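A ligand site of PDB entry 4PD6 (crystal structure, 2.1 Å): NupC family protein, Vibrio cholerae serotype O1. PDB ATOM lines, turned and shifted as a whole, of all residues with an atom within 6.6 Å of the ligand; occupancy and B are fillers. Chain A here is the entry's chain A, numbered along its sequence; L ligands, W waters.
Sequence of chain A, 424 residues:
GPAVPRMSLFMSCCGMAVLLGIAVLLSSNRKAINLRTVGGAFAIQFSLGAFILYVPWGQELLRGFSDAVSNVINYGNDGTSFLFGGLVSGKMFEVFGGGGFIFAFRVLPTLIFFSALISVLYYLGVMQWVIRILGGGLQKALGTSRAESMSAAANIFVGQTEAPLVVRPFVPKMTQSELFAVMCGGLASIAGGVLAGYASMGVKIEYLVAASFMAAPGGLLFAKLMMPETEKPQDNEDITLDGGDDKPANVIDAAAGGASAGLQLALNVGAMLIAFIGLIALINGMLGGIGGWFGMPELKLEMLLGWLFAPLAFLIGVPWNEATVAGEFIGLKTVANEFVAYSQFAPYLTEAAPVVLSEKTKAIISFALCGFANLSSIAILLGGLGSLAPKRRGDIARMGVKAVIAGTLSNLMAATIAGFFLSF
The side-chain carboxylate (OE2) of Glu 338 sits at hydrogen-bond distance from an oxygen (O6) of the ligand, 2.7 Å away.
An oxygen (O3) of the ligand is in hydrogen-bond range of the side-chain hydroxyl (OG) of Ser 377, at 2.8 Å.
The side-chain amide nitrogen (NE2) of Gln 160 sits at hydrogen-bond distance from an oxygen (O1) of the ligand (3.1 Å).
O4 of the ligand is in hydrogen-bond range of ND2 of Asn 374 (3.1 Å).
The side-chain hydroxyl (OG) of Ser 377 is in hydrogen-bond range of the side-chain amide nitrogen (NE2) of Gln 160 (3.3 Å).
The backbone NH (N) of Ser 377 sits at hydrogen-bond distance from the side-chain amide oxygen (OD1) of Asn 374 (3.1 Å).
O of Phe 372 sits at hydrogen-bond distance from OG of Ser 377.
The side-chain amide oxygen (OD1) of Asn 374 lies within hydrogen-bond range of the backbone NH (N) of Ser 376.
The side-chain amide oxygen of Asn 374 sits close to the backbone carbonyl oxygen of Ala 336, 3.4 Å away.
The backbone NH (N) of Phe 339 sits at hydrogen-bond distance from the side-chain amide oxygen (OD1) of Asn 337, 3.0 Å away.
The side-chain amide nitrogen (ND2) of Asn 337 lies within hydrogen-bond range of the side-chain sulfur (SD) of Met 272 (3.6 Å).
The side-chain amide oxygen (OD1) of Asn 337 sits at hydrogen-bond distance from the backbone NH (N) of Val 340, 3.0 Å away.
Ala 191 touches the ligand.
Val 194 touches the ligand.
Tyr 198 touches the ligand (OH to O6, 3.6 Å).
CD1 of Leu 265 touches C3 of the ligand (3.7 Å).
CB of Asn 337 touches O4 of the ligand, 3.9 Å away.
Phe 339 touches the ligand.
Phe 372 touches the ligand.
CD1 of Ile 380 touches O3 of the ligand, 3.2 Å away.
Hydrophobic or aromatic side chains that line the ligand: Ala 191, Val 194, Leu 265, Phe 339, Phe 372 and Ile 380.
Of the 27 residues printed, 12 come within 4 Å of the ligand.
Water W1 bridges OD1 of Asn 374 (2.7 Å) and O3 of the ligand (2.9 Å).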
ATOM      1  N   VAL A 158     -14.103   2.883  -5.865  1.00  0.00           N
ATOM      2  CA  VAL A 158     -14.929   3.183  -4.689  1.00  0.00           C
ATOM      3  C   VAL A 158     -15.123   4.695  -4.488  1.00  0.00           C
ATOM      4  O   VAL A 158     -14.482   5.507  -5.153  1.00  0.00           O
ATOM      5  CB  VAL A 158     -14.336   2.584  -3.403  1.00  0.00           C
ATOM      6  CG1 VAL A 158     -14.284   1.065  -3.512  1.00  0.00           C
ATOM      7  CG2 VAL A 158     -12.957   3.144  -3.139  1.00  0.00           C
ATOM      8  N   GLY A 159     -16.008   5.052  -3.565  1.00  0.00           N
ATOM      9  CA  GLY A 159     -16.409   6.431  -3.361  1.00  0.00           C
ATOM     10  C   GLY A 159     -15.402   7.293  -2.624  1.00  0.00           C
ATOM     11  O   GLY A 159     -14.422   6.792  -2.059  1.00  0.00           O
ATOM     12  N   GLN A 160     -15.670   8.591  -2.623  1.00  0.00           N
ATOM     13  CA  GLN A 160     -14.738   9.604  -2.119  1.00  0.00           C
ATOM     14  C   GLN A 160     -14.333   9.440  -0.667  1.00  0.00           C
ATOM     15  O   GLN A 160     -13.253   9.866  -0.258  1.00  0.00           O
ATOM     16  CB  GLN A 160     -15.334  11.009  -2.327  1.00  0.00           C
ATOM     17  CG  GLN A 160     -16.699  11.210  -1.680  1.00  0.00           C
ATOM     18  CD  GLN A 160     -17.347  12.512  -2.097  1.00  0.00           C
ATOM     19  OE1 GLN A 160     -16.690  13.416  -2.600  1.00  0.00           O
ATOM     20  NE2 GLN A 160     -18.666  12.611  -1.903  1.00  0.00           N
ATOM     21  N   THR A 161     -15.199   8.839   0.147  1.00  0.00           N
ATOM     22  CA  THR A 161     -14.880   8.633   1.554  1.00  0.00           C
ATOM     23  C   THR A 161     -14.279   7.247   1.792  1.00  0.00           C
ATOM     24  O   THR A 161     -13.733   6.985   2.872  1.00  0.00           O
ATOM     25  CB  THR A 161     -16.122   8.807   2.453  1.00  0.00           C
ATOM     26  OG1 THR A 161     -17.171   7.937   2.014  1.00  0.00           O
ATOM     27  CG2 THR A 161     -16.619  10.245   2.410  1.00  0.00           C
ATOM     28  N   GLU A 162     -14.369   6.377   0.798  1.00  0.00           N
ATOM     29  CA  GLU A 162     -13.840   5.019   0.934  1.00  0.00           C
ATOM     30  C   GLU A 162     -12.421   4.889   0.379  1.00  0.00           C
ATOM     31  O   GLU A 162     -11.587   4.194   0.959  1.00  0.00           O
ATOM     32  CB  GLU A 162     -14.754   4.011   0.228  1.00  0.00           C
ATOM     33  CG  GLU A 162     -16.026   3.667   0.998  1.00  0.00           C
ATOM     34  CD  GLU A 162     -17.104   4.723   0.850  1.00  0.00           C
ATOM     35  OE1 GLU A 162     -17.068   5.480  -0.144  1.00  0.00           O
ATOM     36  OE2 GLU A 162     -17.990   4.790   1.736  1.00  0.00           O
ATOM     37  N   ILE A 190     -16.753   8.713  -9.346  1.00  0.00           N
ATOM     38  CA  ILE A 190     -17.960   8.211  -8.686  1.00  0.00           C
ATOM     39  C   ILE A 190     -17.597   6.982  -7.853  1.00  0.00           C
ATOM     40  O   ILE A 190     -16.566   6.976  -7.167  1.00  0.00           O
ATOM     41  CB  ILE A 190     -19.078   7.867  -9.701  1.00  0.00           C
ATOM     42  CG1 ILE A 190     -18.543   6.999 -10.832  1.00  0.00           C
ATOM     43  CG2 ILE A 190     -19.688   9.141 -10.269  1.00  0.00           C
ATOM     44  CD1 ILE A 190     -19.633   6.398 -11.699  1.00  0.00           C
ATOM     45  N   ALA A 191     -18.437   5.947  -7.893  1.00  0.00           N
ATOM     46  CA  ALA A 191     -18.171   4.705  -7.178  1.00  0.00           C
ATOM     47  C   ALA A 191     -18.808   3.517  -7.896  1.00  0.00           C
ATOM     48  O   ALA A 191     -19.762   3.681  -8.646  1.00  0.00           O
ATOM     49  CB  ALA A 191     -18.681   4.799  -5.742  1.00  0.00           C
ATOM     50  N   GLY A 192     -18.281   2.326  -7.626  1.00  0.00           N
ATOM     51  CA  GLY A 192     -18.749   1.107  -8.259  1.00  0.00           C
ATOM     52  C   GLY A 192     -20.237   0.867  -8.070  1.00  0.00           C
ATOM     53  O   GLY A 192     -20.931   0.485  -9.007  1.00  0.00           O
ATOM     54  N   GLY A 193     -20.722   1.111  -6.859  1.00  0.00           N
ATOM     55  CA  GLY A 193     -22.123   0.919  -6.544  1.00  0.00           C
ATOM     56  C   GLY A 193     -23.070   1.740  -7.411  1.00  0.00           C
ATOM     57  O   GLY A 193     -23.955   1.190  -8.075  1.00  0.00           O
ATOM     58  N   VAL A 194     -22.887   3.055  -7.420  1.00  0.00           N
ATOM     59  CA  VAL A 194     -23.763   3.940  -8.180  1.00  0.00           C
ATOM     60  C   VAL A 194     -23.518   3.843  -9.684  1.00  0.00           C
ATOM     61  O   VAL A 194     -24.422   4.128 -10.472  1.00  0.00           O
ATOM     62  CB  VAL A 194     -23.611   5.408  -7.726  1.00  0.00           C
ATOM     63  CG1 VAL A 194     -24.053   5.565  -6.278  1.00  0.00           C
ATOM     64  CG2 VAL A 194     -22.175   5.893  -7.910  1.00  0.00           C
ATOM     65  N   TYR A 198     -26.379   3.707 -12.302  1.00  0.00           N
ATOM     66  CA  TYR A 198     -26.511   4.522 -13.504  1.00  0.00           C
ATOM     67  C   TYR A 198     -26.605   3.654 -14.752  1.00  0.00           C
ATOM     68  O   TYR A 198     -27.318   3.988 -15.693  1.00  0.00           O
ATOM     69  CB  TYR A 198     -25.336   5.507 -13.624  1.00  0.00           C
ATOM     70  CG  TYR A 198     -25.217   6.447 -12.443  1.00  0.00           C
ATOM     71  CD1 TYR A 198     -26.349   6.855 -11.754  1.00  0.00           C
ATOM     72  CD2 TYR A 198     -23.981   6.908 -12.023  1.00  0.00           C
ATOM     73  CE1 TYR A 198     -26.262   7.708 -10.678  1.00  0.00           C
ATOM     74  CE2 TYR A 198     -23.881   7.766 -10.933  1.00  0.00           C
ATOM     75  CZ  TYR A 198     -25.025   8.161 -10.269  1.00  0.00           C
ATOM     76  OH  TYR A 198     -24.941   9.005  -9.188  1.00  0.00           O
ATOM     77  N   LEU A 265     -26.609   3.317   2.102  1.00  0.00           N
ATOM     78  CA  LEU A 265     -26.443   4.159   0.926  1.00  0.00           C
ATOM     79  C   LEU A 265     -27.715   4.182   0.101  1.00  0.00           C
ATOM     80  O   LEU A 265     -28.179   5.233  -0.326  1.00  0.00           O
ATOM     81  CB  LEU A 265     -25.261   3.667   0.083  1.00  0.00           C
ATOM     82  CG  LEU A 265     -24.997   4.429  -1.220  1.00  0.00           C
ATOM     83  CD1 LEU A 265     -24.671   5.887  -0.922  1.00  0.00           C
ATOM     84  CD2 LEU A 265     -23.875   3.775  -2.014  1.00  0.00           C
ATOM     85  N   VAL A 269     -29.950   7.429  -0.727  1.00  0.00           N
ATOM     86  CA  VAL A 269     -30.110   7.851  -2.112  1.00  0.00           C
ATOM     87  C   VAL A 269     -31.596   7.925  -2.449  1.00  0.00           C
ATOM     88  O   VAL A 269     -32.053   8.879  -3.085  1.00  0.00           O
ATOM     89  CB  VAL A 269     -29.391   6.903  -3.095  1.00  0.00           C
ATOM     90  CG1 VAL A 269     -29.856   7.160  -4.530  1.00  0.00           C
ATOM     91  CG2 VAL A 269     -27.881   7.062  -2.974  1.00  0.00           C
ATOM     92  N   MET A 272     -33.105  10.974  -0.731  1.00  0.00           N
ATOM     93  CA  MET A 272     -32.622  12.173  -1.393  1.00  0.00           C
ATOM     94  C   MET A 272     -33.383  12.424  -2.695  1.00  0.00           C
ATOM     95  O   MET A 272     -33.738  13.561  -3.003  1.00  0.00           O
ATOM     96  CB  MET A 272     -31.114  12.060  -1.669  1.00  0.00           C
ATOM     97  CG  MET A 272     -30.517  13.213  -2.474  1.00  0.00           C
ATOM     98  SD  MET A 272     -30.670  13.005  -4.262  1.00  0.00           S
ATOM     99  CE  MET A 272     -29.666  11.531  -4.500  1.00  0.00           C
ATOM    100  N   ALA A 336     -26.887  20.392  -7.780  1.00  0.00           N
ATOM    101  CA  ALA A 336     -27.469  19.387  -6.880  1.00  0.00           C
ATOM    102  C   ALA A 336     -26.490  18.229  -6.726  1.00  0.00           C
ATOM    103  O   ALA A 336     -25.600  18.268  -5.873  1.00  0.00           O
ATOM    104  CB  ALA A 336     -28.812  18.902  -7.419  1.00  0.00           C
ATOM    105  N   ASN A 337     -26.665  17.191  -7.546  1.00  0.00           N
ATOM    106  CA  ASN A 337     -25.698  16.106  -7.654  1.00  0.00           C
ATOM    107  C   ASN A 337     -25.936  15.305  -8.923  1.00  0.00           C
ATOM    108  O   ASN A 337     -26.940  15.501  -9.612  1.00  0.00           O
ATOM    109  CB  ASN A 337     -25.751  15.181  -6.420  1.00  0.00           C
ATOM    110  CG  ASN A 337     -27.113  14.550  -6.216  1.00  0.00           C
ATOM    111  OD1 ASN A 337     -27.550  13.715  -7.005  1.00  0.00           O
ATOM    112  ND2 ASN A 337     -27.789  14.942  -5.131  1.00  0.00           N
ATOM    113  N   GLU A 338     -25.025  14.387  -9.231  1.00  0.00           N
ATOM    114  CA  GLU A 338     -25.071  13.677 -10.501  1.00  0.00           C
ATOM    115  C   GLU A 338     -26.182  12.627 -10.556  1.00  0.00           C
ATOM    116  O   GLU A 338     -26.651  12.284 -11.645  1.00  0.00           O
ATOM    117  CB  GLU A 338     -23.716  13.026 -10.787  1.00  0.00           C
ATOM    118  CG  GLU A 338     -23.517  11.645 -10.195  1.00  0.00           C
ATOM    119  CD  GLU A 338     -23.400  11.654  -8.675  1.00  0.00           C
ATOM    120  OE1 GLU A 338     -23.165  12.732  -8.096  1.00  0.00           O
ATOM    121  OE2 GLU A 338     -23.540  10.566  -8.061  1.00  0.00           O
ATOM    122  N   PHE A 339     -26.605  12.120  -9.408  1.00  0.00           N
ATOM    123  CA  PHE A 339     -27.670  11.122  -9.385  1.00  0.00           C
ATOM    124  C   PHE A 339     -28.984  11.745  -9.849  1.00  0.00           C
ATOM    125  O   PHE A 339     -29.701  11.182 -10.676  1.00  0.00           O
ATOM    126  CB  PHE A 339     -27.828  10.510  -7.998  1.00  0.00           C
ATOM    127  CG  PHE A 339     -28.187   9.048  -8.009  1.00  0.00           C
ATOM    128  CD1 PHE A 339     -27.391   8.117  -7.369  1.00  0.00           C
ATOM    129  CD2 PHE A 339     -29.309   8.614  -8.702  1.00  0.00           C
ATOM    130  CE1 PHE A 339     -27.719   6.770  -7.398  1.00  0.00           C
ATOM    131  CE2 PHE A 339     -29.636   7.267  -8.731  1.00  0.00           C
ATOM    132  CZ  PHE A 339     -28.842   6.344  -8.079  1.00  0.00           C
ATOM    133  N   VAL A 340     -29.305  12.916  -9.293  1.00  0.00           N
ATOM    134  CA  VAL A 340     -30.479  13.675  -9.714  1.00  0.00           C
ATOM    135  C   VAL A 340     -30.378  14.025 -11.196  1.00  0.00           C
ATOM    136  O   VAL A 340     -31.366  13.930 -11.938  1.00  0.00           O
ATOM    137  CB  VAL A 340     -30.649  14.966  -8.878  1.00  0.00           C
ATOM    138  CG1 VAL A 340     -31.793  15.802  -9.429  1.00  0.00           C
ATOM    139  CG2 VAL A 340     -30.902  14.626  -7.430  1.00  0.00           C
ATOM    140  N   GLY A 371     -19.310  12.254 -11.982  1.00  0.00           N
ATOM    141  CA  GLY A 371     -18.471  12.707 -10.896  1.00  0.00           C
ATOM    142  C   GLY A 371     -19.265  13.149  -9.680  1.00  0.00           C
ATOM    143  O   GLY A 371     -20.409  13.565  -9.805  1.00  0.00           O
ATOM    144  N   PHE A 372     -18.651  13.046  -8.502  1.00  0.00           N
ATOM    145  CA  PHE A 372     -19.285  13.473  -7.256  1.00  0.00           C
ATOM    146  C   PHE A 372     -19.068  14.971  -7.002  1.00  0.00           C
ATOM    147  O   PHE A 372     -19.360  15.470  -5.917  1.00  0.00           O
ATOM    148  CB  PHE A 372     -18.748  12.666  -6.060  1.00  0.00           C
ATOM    149  CG  PHE A 372     -19.265  11.250  -6.001  1.00  0.00           C
ATOM    150  CD1 PHE A 372     -20.238  10.811  -6.871  1.00  0.00           C
ATOM    151  CD2 PHE A 372     -18.767  10.372  -5.053  1.00  0.00           C
ATOM    152  CE1 PHE A 372     -20.711   9.516  -6.817  1.00  0.00           C
ATOM    153  CE2 PHE A 372     -19.236   9.072  -4.986  1.00  0.00           C
ATOM    154  CZ  PHE A 372     -20.206   8.641  -5.862  1.00  0.00           C
ATOM    155  N   ALA A 373     -18.556  15.671  -8.012  1.00  0.00           N
ATOM    156  CA  ALA A 373     -18.238  17.084  -7.874  1.00  0.00           C
ATOM    157  C   ALA A 373     -19.498  17.925  -7.724  1.00  0.00           C
ATOM    158  O   ALA A 373     -20.157  18.259  -8.715  1.00  0.00           O
ATOM    159  CB  ALA A 373     -17.396  17.566  -9.055  1.00  0.00           C
ATOM    160  N   ASN A 374     -19.836  18.246  -6.481  1.00  0.00           N
ATOM    161  CA  ASN A 374     -20.897  19.193  -6.161  1.00  0.00           C
ATOM    162  C   ASN A 374     -20.678  19.684  -4.733  1.00  0.00           C
ATOM    163  O   ASN A 374     -19.921  19.064  -3.986  1.00  0.00           O
ATOM    164  CB  ASN A 374     -22.294  18.560  -6.321  1.00  0.00           C
ATOM    165  CG  ASN A 374     -22.510  17.363  -5.409  1.00  0.00           C
ATOM    166  OD1 ASN A 374     -22.737  17.517  -4.214  1.00  0.00           O
ATOM    167  ND2 ASN A 374     -22.438  16.169  -5.982  1.00  0.00           N
ATOM    168  N   SER A 376     -22.482  19.721  -2.028  1.00  0.00           N
ATOM    169  CA  SER A 376     -22.923  18.833  -0.950  1.00  0.00           C
ATOM    170  C   SER A 376     -21.897  17.750  -0.629  1.00  0.00           C
ATOM    171  O   SER A 376     -21.889  17.214   0.488  1.00  0.00           O
ATOM    172  CB  SER A 376     -24.257  18.185  -1.304  1.00  0.00           C
ATOM    173  OG  SER A 376     -25.299  19.142  -1.232  1.00  0.00           O
ATOM    174  N   SER A 377     -21.043  17.432  -1.582  1.00  0.00           N
ATOM    175  CA  SER A 377     -20.003  16.428  -1.377  1.00  0.00           C
ATOM    176  C   SER A 377     -18.934  16.910  -0.401  1.00  0.00           C
ATOM    177  O   SER A 377     -18.199  16.103   0.173  1.00  0.00           O
ATOM    178  CB  SER A 377     -19.356  16.030  -2.703  1.00  0.00           C
ATOM    179  OG  SER A 377     -20.181  15.157  -3.447  1.00  0.00           O
ATOM    180  N   ILE A 378     -18.848  18.221  -0.205  1.00  0.00           N
ATOM    181  CA  ILE A 378     -17.915  18.789   0.762  1.00  0.00           C
ATOM    182  C   ILE A 378     -18.250  18.327   2.179  1.00  0.00           C
ATOM    183  O   ILE A 378     -17.368  17.926   2.935  1.00  0.00           O
ATOM    184  CB  ILE A 378     -17.924  20.333   0.709  1.00  0.00           C
ATOM    185  CG1 ILE A 378     -17.496  20.832  -0.667  1.00  0.00           C
ATOM    186  CG2 ILE A 378     -17.027  20.904   1.792  1.00  0.00           C
ATOM    187  CD1 ILE A 378     -17.586  22.338  -0.829  1.00  0.00           C
ATOM    188  N   ILE A 380     -19.819  15.709   2.970  1.00  0.00           N
ATOM    189  CA  ILE A 380     -19.570  14.272   3.014  1.00  0.00           C
ATOM    190  C   ILE A 380     -18.090  13.991   3.229  1.00  0.00           C
ATOM    191  O   ILE A 380     -17.714  13.110   4.008  1.00  0.00           O
ATOM    192  CB  ILE A 380     -20.071  13.579   1.730  1.00  0.00           C
ATOM    193  CG1 ILE A 380     -21.597  13.674   1.661  1.00  0.00           C
ATOM    194  CG2 ILE A 380     -19.624  12.131   1.682  1.00  0.00           C
ATOM    195  CD1 ILE A 380     -22.189  13.057   0.429  1.00  0.00           C
HETATM  196  N1  LIG L   1     -22.243   9.618  -2.587  1.00  0.00           N
HETATM  197  C1  LIG L   1     -21.073   9.368  -1.902  1.00  0.00           C
HETATM  198  N2  LIG L   1     -20.608   8.088  -2.007  1.00  0.00           N
HETATM  199  C2  LIG L   1     -21.183   7.051  -2.715  1.00  0.00           C
HETATM  200  C3  LIG L   1     -22.390   7.386  -3.402  1.00  0.00           C
HETATM  201  C4  LIG L   1     -22.872   8.636  -3.311  1.00  0.00           C
HETATM  202  O1  LIG L   1     -20.485  10.218  -1.243  1.00  0.00           O
HETATM  203  O2  LIG L   1     -20.641   5.942  -2.719  1.00  0.00           O
HETATM  204  C5  LIG L   1     -22.803  10.998  -2.507  1.00  0.00           C
HETATM  205  C6  LIG L   1     -22.015  11.991  -3.351  1.00  0.00           C
HETATM  206  C7  LIG L   1     -22.809  11.974  -4.656  1.00  0.00           C
HETATM  207  C8  LIG L   1     -24.242  11.822  -4.171  1.00  0.00           C
HETATM  208  O3  LIG L   1     -22.096  13.268  -2.733  1.00  0.00           O
HETATM  209  O4  LIG L   1     -22.601  13.132  -5.446  1.00  0.00           O
HETATM  210  O5  LIG L   1     -24.133  10.965  -3.002  1.00  0.00           O
HETATM  211  C9  LIG L   1     -25.208  11.210  -5.161  1.00  0.00           C
HETATM  212  O6  LIG L   1     -24.698  10.003  -5.705  1.00  0.00           O
HETATM  213  O   HOH W   1     -23.921  15.454  -3.009  1.00  0.00           O
